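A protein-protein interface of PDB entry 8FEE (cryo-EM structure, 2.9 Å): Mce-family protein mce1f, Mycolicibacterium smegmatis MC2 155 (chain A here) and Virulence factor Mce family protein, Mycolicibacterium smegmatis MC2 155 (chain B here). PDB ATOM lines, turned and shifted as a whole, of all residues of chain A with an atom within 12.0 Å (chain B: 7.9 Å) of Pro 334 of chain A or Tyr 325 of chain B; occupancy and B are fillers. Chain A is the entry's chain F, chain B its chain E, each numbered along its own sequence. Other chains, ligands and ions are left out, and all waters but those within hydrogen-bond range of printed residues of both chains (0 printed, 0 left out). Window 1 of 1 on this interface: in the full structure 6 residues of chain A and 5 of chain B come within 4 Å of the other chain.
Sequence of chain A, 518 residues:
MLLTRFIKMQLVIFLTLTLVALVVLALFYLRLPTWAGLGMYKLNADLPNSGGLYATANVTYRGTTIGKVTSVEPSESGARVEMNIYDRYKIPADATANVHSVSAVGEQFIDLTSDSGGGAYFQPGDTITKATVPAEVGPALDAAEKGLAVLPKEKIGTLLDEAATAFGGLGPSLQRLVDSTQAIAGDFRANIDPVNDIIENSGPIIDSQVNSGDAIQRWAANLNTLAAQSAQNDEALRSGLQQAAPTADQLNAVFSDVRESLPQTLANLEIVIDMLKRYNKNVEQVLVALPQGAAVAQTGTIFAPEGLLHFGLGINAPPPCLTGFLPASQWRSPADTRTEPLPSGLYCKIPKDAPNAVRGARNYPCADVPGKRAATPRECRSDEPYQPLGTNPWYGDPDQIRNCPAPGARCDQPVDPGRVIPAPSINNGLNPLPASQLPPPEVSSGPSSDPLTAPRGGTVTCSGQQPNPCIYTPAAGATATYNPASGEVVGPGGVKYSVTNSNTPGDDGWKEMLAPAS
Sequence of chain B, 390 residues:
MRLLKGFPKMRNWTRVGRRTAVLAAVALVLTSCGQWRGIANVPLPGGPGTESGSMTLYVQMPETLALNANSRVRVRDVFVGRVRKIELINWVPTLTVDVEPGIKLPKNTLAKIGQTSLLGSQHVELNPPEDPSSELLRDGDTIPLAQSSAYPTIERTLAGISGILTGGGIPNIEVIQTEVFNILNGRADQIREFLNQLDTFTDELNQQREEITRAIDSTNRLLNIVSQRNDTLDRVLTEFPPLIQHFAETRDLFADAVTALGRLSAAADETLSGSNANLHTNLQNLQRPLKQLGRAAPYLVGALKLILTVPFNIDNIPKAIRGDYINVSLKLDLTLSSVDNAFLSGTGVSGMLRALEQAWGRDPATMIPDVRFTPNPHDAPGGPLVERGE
Of chain B, only Tyr 325 (3.5 Å) comes within 4 Å of Pro 334 of chain A.
Printed residues of chain A within 4 Å of Tyr 325 of chain B: Arg 332 (3.1 Å) and Pro 334 (3.5 Å).
No residue of chain B comes within 4 Å of Ser 333 of chain A.
No residue of chain B comes within 4 Å of Ala 335 of chain A.
No residue of chain A comes within 4 Å of Ile 321 of chain B.
Asp 324 of chain B touches just one residue of chain A: Arg 332 (3.0 Å).
No residue of chain A comes within 4 Å of Ile 326 of chain B.
Of the printed residues of chain B, Arg 332 of chain A touches Asp 324 and Tyr 325.
Of the printed residues of chain A, Arg 322 of chain B touches Asp 336 (3.98 Å) and Thr 337 (3.7 Å).
Printed residues of chain B within 4 Å of Thr 337 of chain A: Arg 322 (3.7 Å).
The nearest residue of chain B that does not touch Pro 334 of chain A is Arg 322 of chain B (5.1 Å).
The nearest printed residue of chain B that does not touch Asp 336 of chain A is Gly 323 of chain B (5.1 Å).
The backbone carbonyl oxygen of Lys 319 of chain B is in hydrogen-bond range of the guanidinium group of Arg 322 of chain B (3.0 Å).
The backbone carbonyl oxygen of Arg 338 of chain A sits at hydrogen-bond distance from the guanidinium group of Arg 332 of chain A (3.0 Å).
The guanidinium group of Arg 332 of chain A lies within salt-bridge range of the side-chain carboxylate of Glu 340 of chain A (3.8 Å).
The guanidinium group (NH2) of Arg 332 of chain A lies within salt-bridge range of the side-chain carboxylate (OD2) of Asp 324 of chain B, at 3.0 Å.
The backbone carbonyl oxygen (O) of Arg 332 of chain A is in hydrogen-bond range of the side-chain hydroxyl (OH) of Tyr 325 of chain B.
Of the 16 printed residues of chain A, 4 touch a printed residue of chain B.
Of the 10 printed residues of chain B, 3 touch a printed residue of chain A.
Hydrophobic or aromatic side chains of chain B that line the printed part of chain A: Tyr 325.
Among the printed residues, 5 pairs touch across the chains.
Tyr 325 of chain B touches Pro 334 of chain A.
Asp 336 of chain A touches Arg 322 of chain B (O to O, 3.98 Å).
Arg 322 of chain B touches Thr 337 of chain A (O to CA, 3.7 Å).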
ATOM      1  N   LEU A 322     -20.636 -23.011 -27.452  1.00  0.00           N
ATOM      2  CA  LEU A 322     -19.955 -22.136 -26.507  1.00  0.00           C
ATOM      3  C   LEU A 322     -18.462 -22.421 -26.402  1.00  0.00           C
ATOM      4  O   LEU A 322     -17.804 -21.894 -25.500  1.00  0.00           O
ATOM      5  CB  LEU A 322     -20.608 -22.245 -25.127  1.00  0.00           C
ATOM      6  CG  LEU A 322     -22.119 -22.008 -25.072  1.00  0.00           C
ATOM      7  CD1 LEU A 322     -22.621 -22.078 -23.639  1.00  0.00           C
ATOM      8  CD2 LEU A 322     -22.481 -20.674 -25.701  1.00  0.00           C
ATOM      9  N   LEU A 326     -16.443 -16.560 -25.195  1.00  0.00           N
ATOM     10  CA  LEU A 326     -16.300 -16.064 -23.835  1.00  0.00           C
ATOM     11  C   LEU A 326     -17.059 -16.965 -22.862  1.00  0.00           C
ATOM     12  O   LEU A 326     -18.169 -17.414 -23.171  1.00  0.00           O
ATOM     13  CB  LEU A 326     -16.821 -14.631 -23.740  1.00  0.00           C
ATOM     14  CG  LEU A 326     -16.447 -13.796 -22.517  1.00  0.00           C
ATOM     15  CD1 LEU A 326     -14.954 -13.524 -22.491  1.00  0.00           C
ATOM     16  CD2 LEU A 326     -17.230 -12.495 -22.503  1.00  0.00           C
ATOM     17  N   PRO A 327     -16.485 -17.263 -21.696  1.00  0.00           N
ATOM     18  CA  PRO A 327     -17.196 -18.090 -20.714  1.00  0.00           C
ATOM     19  C   PRO A 327     -18.448 -17.392 -20.204  1.00  0.00           C
ATOM     20  O   PRO A 327     -18.542 -16.164 -20.202  1.00  0.00           O
ATOM     21  CB  PRO A 327     -16.167 -18.280 -19.595  1.00  0.00           C
ATOM     22  CG  PRO A 327     -14.849 -18.025 -20.241  1.00  0.00           C
ATOM     23  CD  PRO A 327     -15.102 -16.981 -21.280  1.00  0.00           C
ATOM     24  N   ALA A 328     -19.416 -18.202 -19.766  1.00  0.00           N
ATOM     25  CA  ALA A 328     -20.684 -17.664 -19.278  1.00  0.00           C
ATOM     26  C   ALA A 328     -20.485 -16.776 -18.057  1.00  0.00           C
ATOM     27  O   ALA A 328     -21.140 -15.735 -17.926  1.00  0.00           O
ATOM     28  CB  ALA A 328     -21.648 -18.805 -18.958  1.00  0.00           C
ATOM     29  N   SER A 329     -19.590 -17.172 -17.149  1.00  0.00           N
ATOM     30  CA  SER A 329     -19.319 -16.378 -15.956  1.00  0.00           C
ATOM     31  C   SER A 329     -18.712 -15.018 -16.279  1.00  0.00           C
ATOM     32  O   SER A 329     -18.700 -14.135 -15.414  1.00  0.00           O
ATOM     33  CB  SER A 329     -18.392 -17.149 -15.016  1.00  0.00           C
ATOM     34  OG  SER A 329     -17.920 -16.318 -13.970  1.00  0.00           O
ATOM     35  N   GLN A 330     -18.206 -14.829 -17.496  1.00  0.00           N
ATOM     36  CA  GLN A 330     -17.619 -13.568 -17.923  1.00  0.00           C
ATOM     37  C   GLN A 330     -18.595 -12.688 -18.693  1.00  0.00           C
ATOM     38  O   GLN A 330     -18.188 -11.649 -19.222  1.00  0.00           O
ATOM     39  CB  GLN A 330     -16.373 -13.829 -18.771  1.00  0.00           C
ATOM     40  CG  GLN A 330     -15.330 -14.701 -18.094  1.00  0.00           C
ATOM     41  CD  GLN A 330     -14.810 -14.099 -16.805  1.00  0.00           C
ATOM     42  OE1 GLN A 330     -13.976 -13.194 -16.821  1.00  0.00           O
ATOM     43  NE2 GLN A 330     -15.300 -14.602 -15.676  1.00  0.00           N
ATOM     44  N   TRP A 331     -19.864 -13.078 -18.780  1.00  0.00           N
ATOM     45  CA  TRP A 331     -20.857 -12.232 -19.425  1.00  0.00           C
ATOM     46  C   TRP A 331     -21.152 -11.002 -18.569  1.00  0.00           C
ATOM     47  O   TRP A 331     -20.934 -10.986 -17.354  1.00  0.00           O
ATOM     48  CB  TRP A 331     -22.155 -13.002 -19.674  1.00  0.00           C
ATOM     49  CG  TRP A 331     -22.051 -14.122 -20.672  1.00  0.00           C
ATOM     50  CD1 TRP A 331     -20.913 -14.677 -21.170  1.00  0.00           C
ATOM     51  CD2 TRP A 331     -23.139 -14.823 -21.285  1.00  0.00           C
ATOM     52  NE1 TRP A 331     -21.221 -15.679 -22.057  1.00  0.00           N
ATOM     53  CE2 TRP A 331     -22.583 -15.789 -22.144  1.00  0.00           C
ATOM     54  CE3 TRP A 331     -24.530 -14.727 -21.189  1.00  0.00           C
ATOM     55  CZ2 TRP A 331     -23.368 -16.652 -22.904  1.00  0.00           C
ATOM     56  CZ3 TRP A 331     -25.307 -15.584 -21.943  1.00  0.00           C
ATOM     57  CH2 TRP A 331     -24.725 -16.534 -22.790  1.00  0.00           C
ATOM     58  N   ARG A 332     -21.659  -9.959 -19.222  1.00  0.00           N
ATOM     59  CA  ARG A 332     -22.017  -8.712 -18.561  1.00  0.00           C
ATOM     60  C   ARG A 332     -23.514  -8.466 -18.681  1.00  0.00           C
ATOM     61  O   ARG A 332     -24.130  -8.799 -19.698  1.00  0.00           O
ATOM     62  CB  ARG A 332     -21.240  -7.529 -19.149  1.00  0.00           C
ATOM     63  CG  ARG A 332     -19.733  -7.645 -18.990  1.00  0.00           C
ATOM     64  CD  ARG A 332     -19.019  -6.346 -19.333  1.00  0.00           C
ATOM     65  NE  ARG A 332     -19.416  -5.812 -20.629  1.00  0.00           N
ATOM     66  CZ  ARG A 332     -20.023  -4.647 -20.804  1.00  0.00           C
ATOM     67  NH1 ARG A 332     -20.301  -3.853 -19.784  1.00  0.00           N
ATOM     68  NH2 ARG A 332     -20.349  -4.263 -22.034  1.00  0.00           N
ATOM     69  N   SER A 333     -24.089  -7.888 -17.628  1.00  0.00           N
ATOM     70  CA  SER A 333     -25.512  -7.593 -17.601  1.00  0.00           C
ATOM     71  C   SER A 333     -25.862  -6.560 -18.674  1.00  0.00           C
ATOM     72  O   SER A 333     -25.040  -5.705 -19.013  1.00  0.00           O
ATOM     73  CB  SER A 333     -25.908  -7.078 -16.217  1.00  0.00           C
ATOM     74  OG  SER A 333     -27.135  -6.373 -16.249  1.00  0.00           O
ATOM     75  N   PRO A 334     -27.076  -6.623 -19.235  1.00  0.00           N
ATOM     76  CA  PRO A 334     -27.439  -5.687 -20.313  1.00  0.00           C
ATOM     77  C   PRO A 334     -27.563  -4.240 -19.868  1.00  0.00           C
ATOM     78  O   PRO A 334     -27.683  -3.361 -20.731  1.00  0.00           O
ATOM     79  CB  PRO A 334     -28.784  -6.230 -20.811  1.00  0.00           C
ATOM     80  CG  PRO A 334     -29.335  -6.988 -19.656  1.00  0.00           C
ATOM     81  CD  PRO A 334     -28.150  -7.597 -18.971  1.00  0.00           C
ATOM     82  N   ALA A 335     -27.549  -3.965 -18.562  1.00  0.00           N
ATOM     83  CA  ALA A 335     -27.717  -2.596 -18.085  1.00  0.00           C
ATOM     84  C   ALA A 335     -26.550  -1.711 -18.505  1.00  0.00           C
ATOM     85  O   ALA A 335     -26.753  -0.558 -18.907  1.00  0.00           O
ATOM     86  CB  ALA A 335     -27.876  -2.588 -16.565  1.00  0.00           C
ATOM     87  N   ASP A 336     -25.327  -2.226 -18.420  1.00  0.00           N
ATOM     88  CA  ASP A 336     -24.133  -1.426 -18.673  1.00  0.00           C
ATOM     89  C   ASP A 336     -24.008  -1.135 -20.164  1.00  0.00           C
ATOM     90  O   ASP A 336     -23.787  -2.046 -20.967  1.00  0.00           O
ATOM     91  CB  ASP A 336     -22.895  -2.157 -18.162  1.00  0.00           C
ATOM     92  CG  ASP A 336     -23.014  -2.558 -16.706  1.00  0.00           C
ATOM     93  OD1 ASP A 336     -23.684  -1.834 -15.941  1.00  0.00           O
ATOM     94  OD2 ASP A 336     -22.436  -3.598 -16.326  1.00  0.00           O
ATOM     95  N   THR A 337     -24.146   0.135 -20.536  1.00  0.00           N
ATOM     96  CA  THR A 337     -23.869   0.587 -21.893  1.00  0.00           C
ATOM     97  C   THR A 337     -22.395   0.904 -22.103  1.00  0.00           C
ATOM     98  O   THR A 337     -22.022   1.393 -23.174  1.00  0.00           O
ATOM     99  CB  THR A 337     -24.713   1.822 -22.232  1.00  0.00           C
ATOM    100  OG1 THR A 337     -24.349   2.905 -21.368  1.00  0.00           O
ATOM    101  CG2 THR A 337     -26.193   1.522 -22.062  1.00  0.00           C
ATOM    102  N   ARG A 338     -21.563   0.644 -21.100  1.00  0.00           N
ATOM    103  CA  ARG A 338     -20.131   0.882 -21.197  1.00  0.00           C
ATOM    104  C   ARG A 338     -19.485  -0.083 -22.185  1.00  0.00           C
ATOM    105  O   ARG A 338     -19.735  -1.292 -22.145  1.00  0.00           O
ATOM    106  CB  ARG A 338     -19.497   0.727 -19.817  1.00  0.00           C
ATOM    107  CG  ARG A 338     -17.995   0.901 -19.770  1.00  0.00           C
ATOM    108  CD  ARG A 338     -17.517   0.781 -18.337  1.00  0.00           C
ATOM    109  NE  ARG A 338     -18.220  -0.292 -17.642  1.00  0.00           N
ATOM    110  CZ  ARG A 338     -18.137  -0.524 -16.340  1.00  0.00           C
ATOM    111  NH1 ARG A 338     -17.394   0.232 -15.548  1.00  0.00           N
ATOM    112  NH2 ARG A 338     -18.821  -1.537 -15.818  1.00  0.00           N
ATOM    113  N   THR A 339     -18.653   0.456 -23.070  1.00  0.00           N
ATOM    114  CA  THR A 339     -17.943  -0.355 -24.044  1.00  0.00           C
ATOM    115  C   THR A 339     -16.718  -0.996 -23.391  1.00  0.00           C
ATOM    116  O   THR A 339     -16.185  -0.503 -22.393  1.00  0.00           O
ATOM    117  CB  THR A 339     -17.530   0.497 -25.247  1.00  0.00           C
ATOM    118  OG1 THR A 339     -18.551   1.463 -25.518  1.00  0.00           O
ATOM    119  CG2 THR A 339     -17.346  -0.367 -26.485  1.00  0.00           C
ATOM    120  N   GLU A 340     -16.279  -2.110 -23.960  1.00  0.00           N
ATOM    121  CA  GLU A 340     -15.111  -2.826 -23.476  1.00  0.00           C
ATOM    122  C   GLU A 340     -14.252  -3.231 -24.665  1.00  0.00           C
ATOM    123  O   GLU A 340     -14.746  -3.298 -25.797  1.00  0.00           O
ATOM    124  CB  GLU A 340     -15.524  -4.062 -22.664  1.00  0.00           C
ATOM    125  CG  GLU A 340     -15.940  -3.749 -21.239  1.00  0.00           C
ATOM    126  CD  GLU A 340     -15.554  -4.847 -20.268  1.00  0.00           C
ATOM    127  OE1 GLU A 340     -14.735  -5.711 -20.645  1.00  0.00           O
ATOM    128  OE2 GLU A 340     -16.066  -4.844 -19.130  1.00  0.00           O
ATOM    129  N   LYS B 319     -26.207   4.827 -30.867  1.00  0.00           N
ATOM    130  CA  LYS B 319     -27.455   4.931 -30.121  1.00  0.00           C
ATOM    131  C   LYS B 319     -28.291   3.657 -30.187  1.00  0.00           C
ATOM    132  O   LYS B 319     -28.920   3.286 -29.192  1.00  0.00           O
ATOM    133  CB  LYS B 319     -28.277   6.124 -30.620  1.00  0.00           C
ATOM    134  CG  LYS B 319     -28.645   6.100 -32.096  1.00  0.00           C
ATOM    135  CD  LYS B 319     -29.347   7.390 -32.484  1.00  0.00           C
ATOM    136  CE  LYS B 319     -29.843   7.368 -33.915  1.00  0.00           C
ATOM    137  NZ  LYS B 319     -30.379   8.693 -34.333  1.00  0.00           N
ATOM    138  N   ALA B 320     -28.317   2.975 -31.334  1.00  0.00           N
ATOM    139  CA  ALA B 320     -29.083   1.737 -31.425  1.00  0.00           C
ATOM    140  C   ALA B 320     -28.418   0.611 -30.643  1.00  0.00           C
ATOM    141  O   ALA B 320     -29.092  -0.125 -29.913  1.00  0.00           O
ATOM    142  CB  ALA B 320     -29.266   1.341 -32.889  1.00  0.00           C
ATOM    143  N   ILE B 321     -27.103   0.464 -30.773  1.00  0.00           N
ATOM    144  CA  ILE B 321     -26.361  -0.610 -30.122  1.00  0.00           C
ATOM    145  C   ILE B 321     -25.753  -0.055 -28.840  1.00  0.00           C
ATOM    146  O   ILE B 321     -24.768   0.689 -28.882  1.00  0.00           O
ATOM    147  CB  ILE B 321     -25.279  -1.188 -31.042  1.00  0.00           C
ATOM    148  CG1 ILE B 321     -25.880  -1.593 -32.387  1.00  0.00           C
ATOM    149  CG2 ILE B 321     -24.616  -2.383 -30.384  1.00  0.00           C
ATOM    150  CD1 ILE B 321     -24.901  -2.283 -33.304  1.00  0.00           C
ATOM    151  N   ARG B 322     -26.328  -0.417 -27.700  1.00  0.00           N
ATOM    152  CA  ARG B 322     -25.857   0.072 -26.404  1.00  0.00           C
ATOM    153  C   ARG B 322     -24.916  -0.942 -25.757  1.00  0.00           C
ATOM    154  O   ARG B 322     -25.145  -1.439 -24.654  1.00  0.00           O
ATOM    155  CB  ARG B 322     -27.040   0.392 -25.494  1.00  0.00           C
ATOM    156  CG  ARG B 322     -28.014   1.409 -26.061  1.00  0.00           C
ATOM    157  CD  ARG B 322     -27.341   2.750 -26.290  1.00  0.00           C
ATOM    158  NE  ARG B 322     -28.218   3.688 -26.981  1.00  0.00           N
ATOM    159  CZ  ARG B 322     -29.129   4.442 -26.380  1.00  0.00           C
ATOM    160  NH1 ARG B 322     -29.308   4.398 -25.070  1.00  0.00           N
ATOM    161  NH2 ARG B 322     -29.880   5.258 -27.112  1.00  0.00           N
ATOM    162  N   GLY B 323     -23.835  -1.242 -26.469  1.00  0.00           N
ATOM    163  CA  GLY B 323     -22.792  -2.090 -25.929  1.00  0.00           C
ATOM    164  C   GLY B 323     -22.918  -3.535 -26.361  1.00  0.00           C
ATOM    165  O   GLY B 323     -22.908  -3.831 -27.560  1.00  0.00           O
ATOM    166  N   ASP B 324     -23.018  -4.449 -25.388  1.00  0.00           N
ATOM    167  CA  ASP B 324     -23.073  -5.872 -25.708  1.00  0.00           C
ATOM    168  C   ASP B 324     -24.312  -6.214 -26.525  1.00  0.00           C
ATOM    169  O   ASP B 324     -24.233  -6.975 -27.494  1.00  0.00           O
ATOM    170  CB  ASP B 324     -23.034  -6.704 -24.426  1.00  0.00           C
ATOM    171  CG  ASP B 324     -21.706  -6.608 -23.710  1.00  0.00           C
ATOM    172  OD1 ASP B 324     -20.710  -6.219 -24.353  1.00  0.00           O
ATOM    173  OD2 ASP B 324     -21.655  -6.926 -22.504  1.00  0.00           O
ATOM    174  N   TYR B 325     -25.463  -5.659 -26.158  1.00  0.00           N
ATOM    175  CA  TYR B 325     -26.744  -6.078 -26.700  1.00  0.00           C
ATOM    176  C   TYR B 325     -27.304  -5.006 -27.626  1.00  0.00           C
ATOM    177  O   TYR B 325     -27.107  -3.809 -27.409  1.00  0.00           O
ATOM    178  CB  TYR B 325     -27.745  -6.376 -25.579  1.00  0.00           C
ATOM    179  CG  TYR B 325     -27.264  -7.393 -24.567  1.00  0.00           C
ATOM    180  CD1 TYR B 325     -26.431  -7.025 -23.521  1.00  0.00           C
ATOM    181  CD2 TYR B 325     -27.651  -8.723 -24.654  1.00  0.00           C
ATOM    182  CE1 TYR B 325     -25.992  -7.953 -22.596  1.00  0.00           C
ATOM    183  CE2 TYR B 325     -27.219  -9.657 -23.731  1.00  0.00           C
ATOM    184  CZ  TYR B 325     -26.391  -9.265 -22.704  1.00  0.00           C
ATOM    185  OH  TYR B 325     -25.958 -10.190 -21.783  1.00  0.00           O
ATOM    186  N   ILE B 326     -28.013  -5.451 -28.662  1.00  0.00           N
ATOM    187  CA  ILE B 326     -28.635  -4.566 -29.639  1.00  0.00           C
ATOM    188  C   ILE B 326     -30.089  -4.352 -29.251  1.00  0.00           C
ATOM    189  O   ILE B 326     -30.831  -5.319 -29.037  1.00  0.00           O
ATOM    190  CB  ILE B 326     -28.530  -5.146 -31.060  1.00  0.00           C
ATOM    191  CG1 ILE B 326     -27.068  -5.375 -31.437  1.00  0.00           C
ATOM    192  CG2 ILE B 326     -29.202  -4.226 -32.064  1.00  0.00           C
ATOM    193  CD1 ILE B 326     -26.884  -6.001 -32.800  1.00  0.00           C
ATOM    194  N   ASN B 327     -30.502  -3.090 -29.166  1.00  0.00           N
ATOM    195  CA  ASN B 327     -31.885  -2.757 -28.848  1.00  0.00           C
ATOM    196  C   ASN B 327     -32.730  -2.784 -30.116  1.00  0.00           C
ATOM    197  O   ASN B 327     -32.430  -2.080 -31.086  1.00  0.00           O
ATOM    198  CB  ASN B 327     -31.963  -1.388 -28.177  1.00  0.00           C
ATOM    199  CG  ASN B 327     -31.294  -1.365 -26.817  1.00  0.00           C
ATOM    200  OD1 ASN B 327     -31.098  -2.407 -26.192  1.00  0.00           O
ATOM    201  ND2 ASN B 327     -30.948  -0.174 -26.349  1.00  0.00           N
ATOM    202  N   VAL B 328     -33.789  -3.592 -30.106  1.00  0.00           N
ATOM    203  CA  VAL B 328     -34.648  -3.788 -31.268  1.00  0.00           C
ATOM    204  C   VAL B 328     -36.102  -3.677 -30.824  1.00  0.00           C
ATOM    205  O   VAL B 328     -36.458  -4.084 -29.712  1.00  0.00           O
ATOM    206  CB  VAL B 328     -34.367  -5.143 -31.961  1.00  0.00           C
ATOM    207  CG1 VAL B 328     -34.758  -6.317 -31.071  1.00  0.00           C
ATOM    208  CG2 VAL B 328     -35.066  -5.221 -33.312  1.00  0.00           C
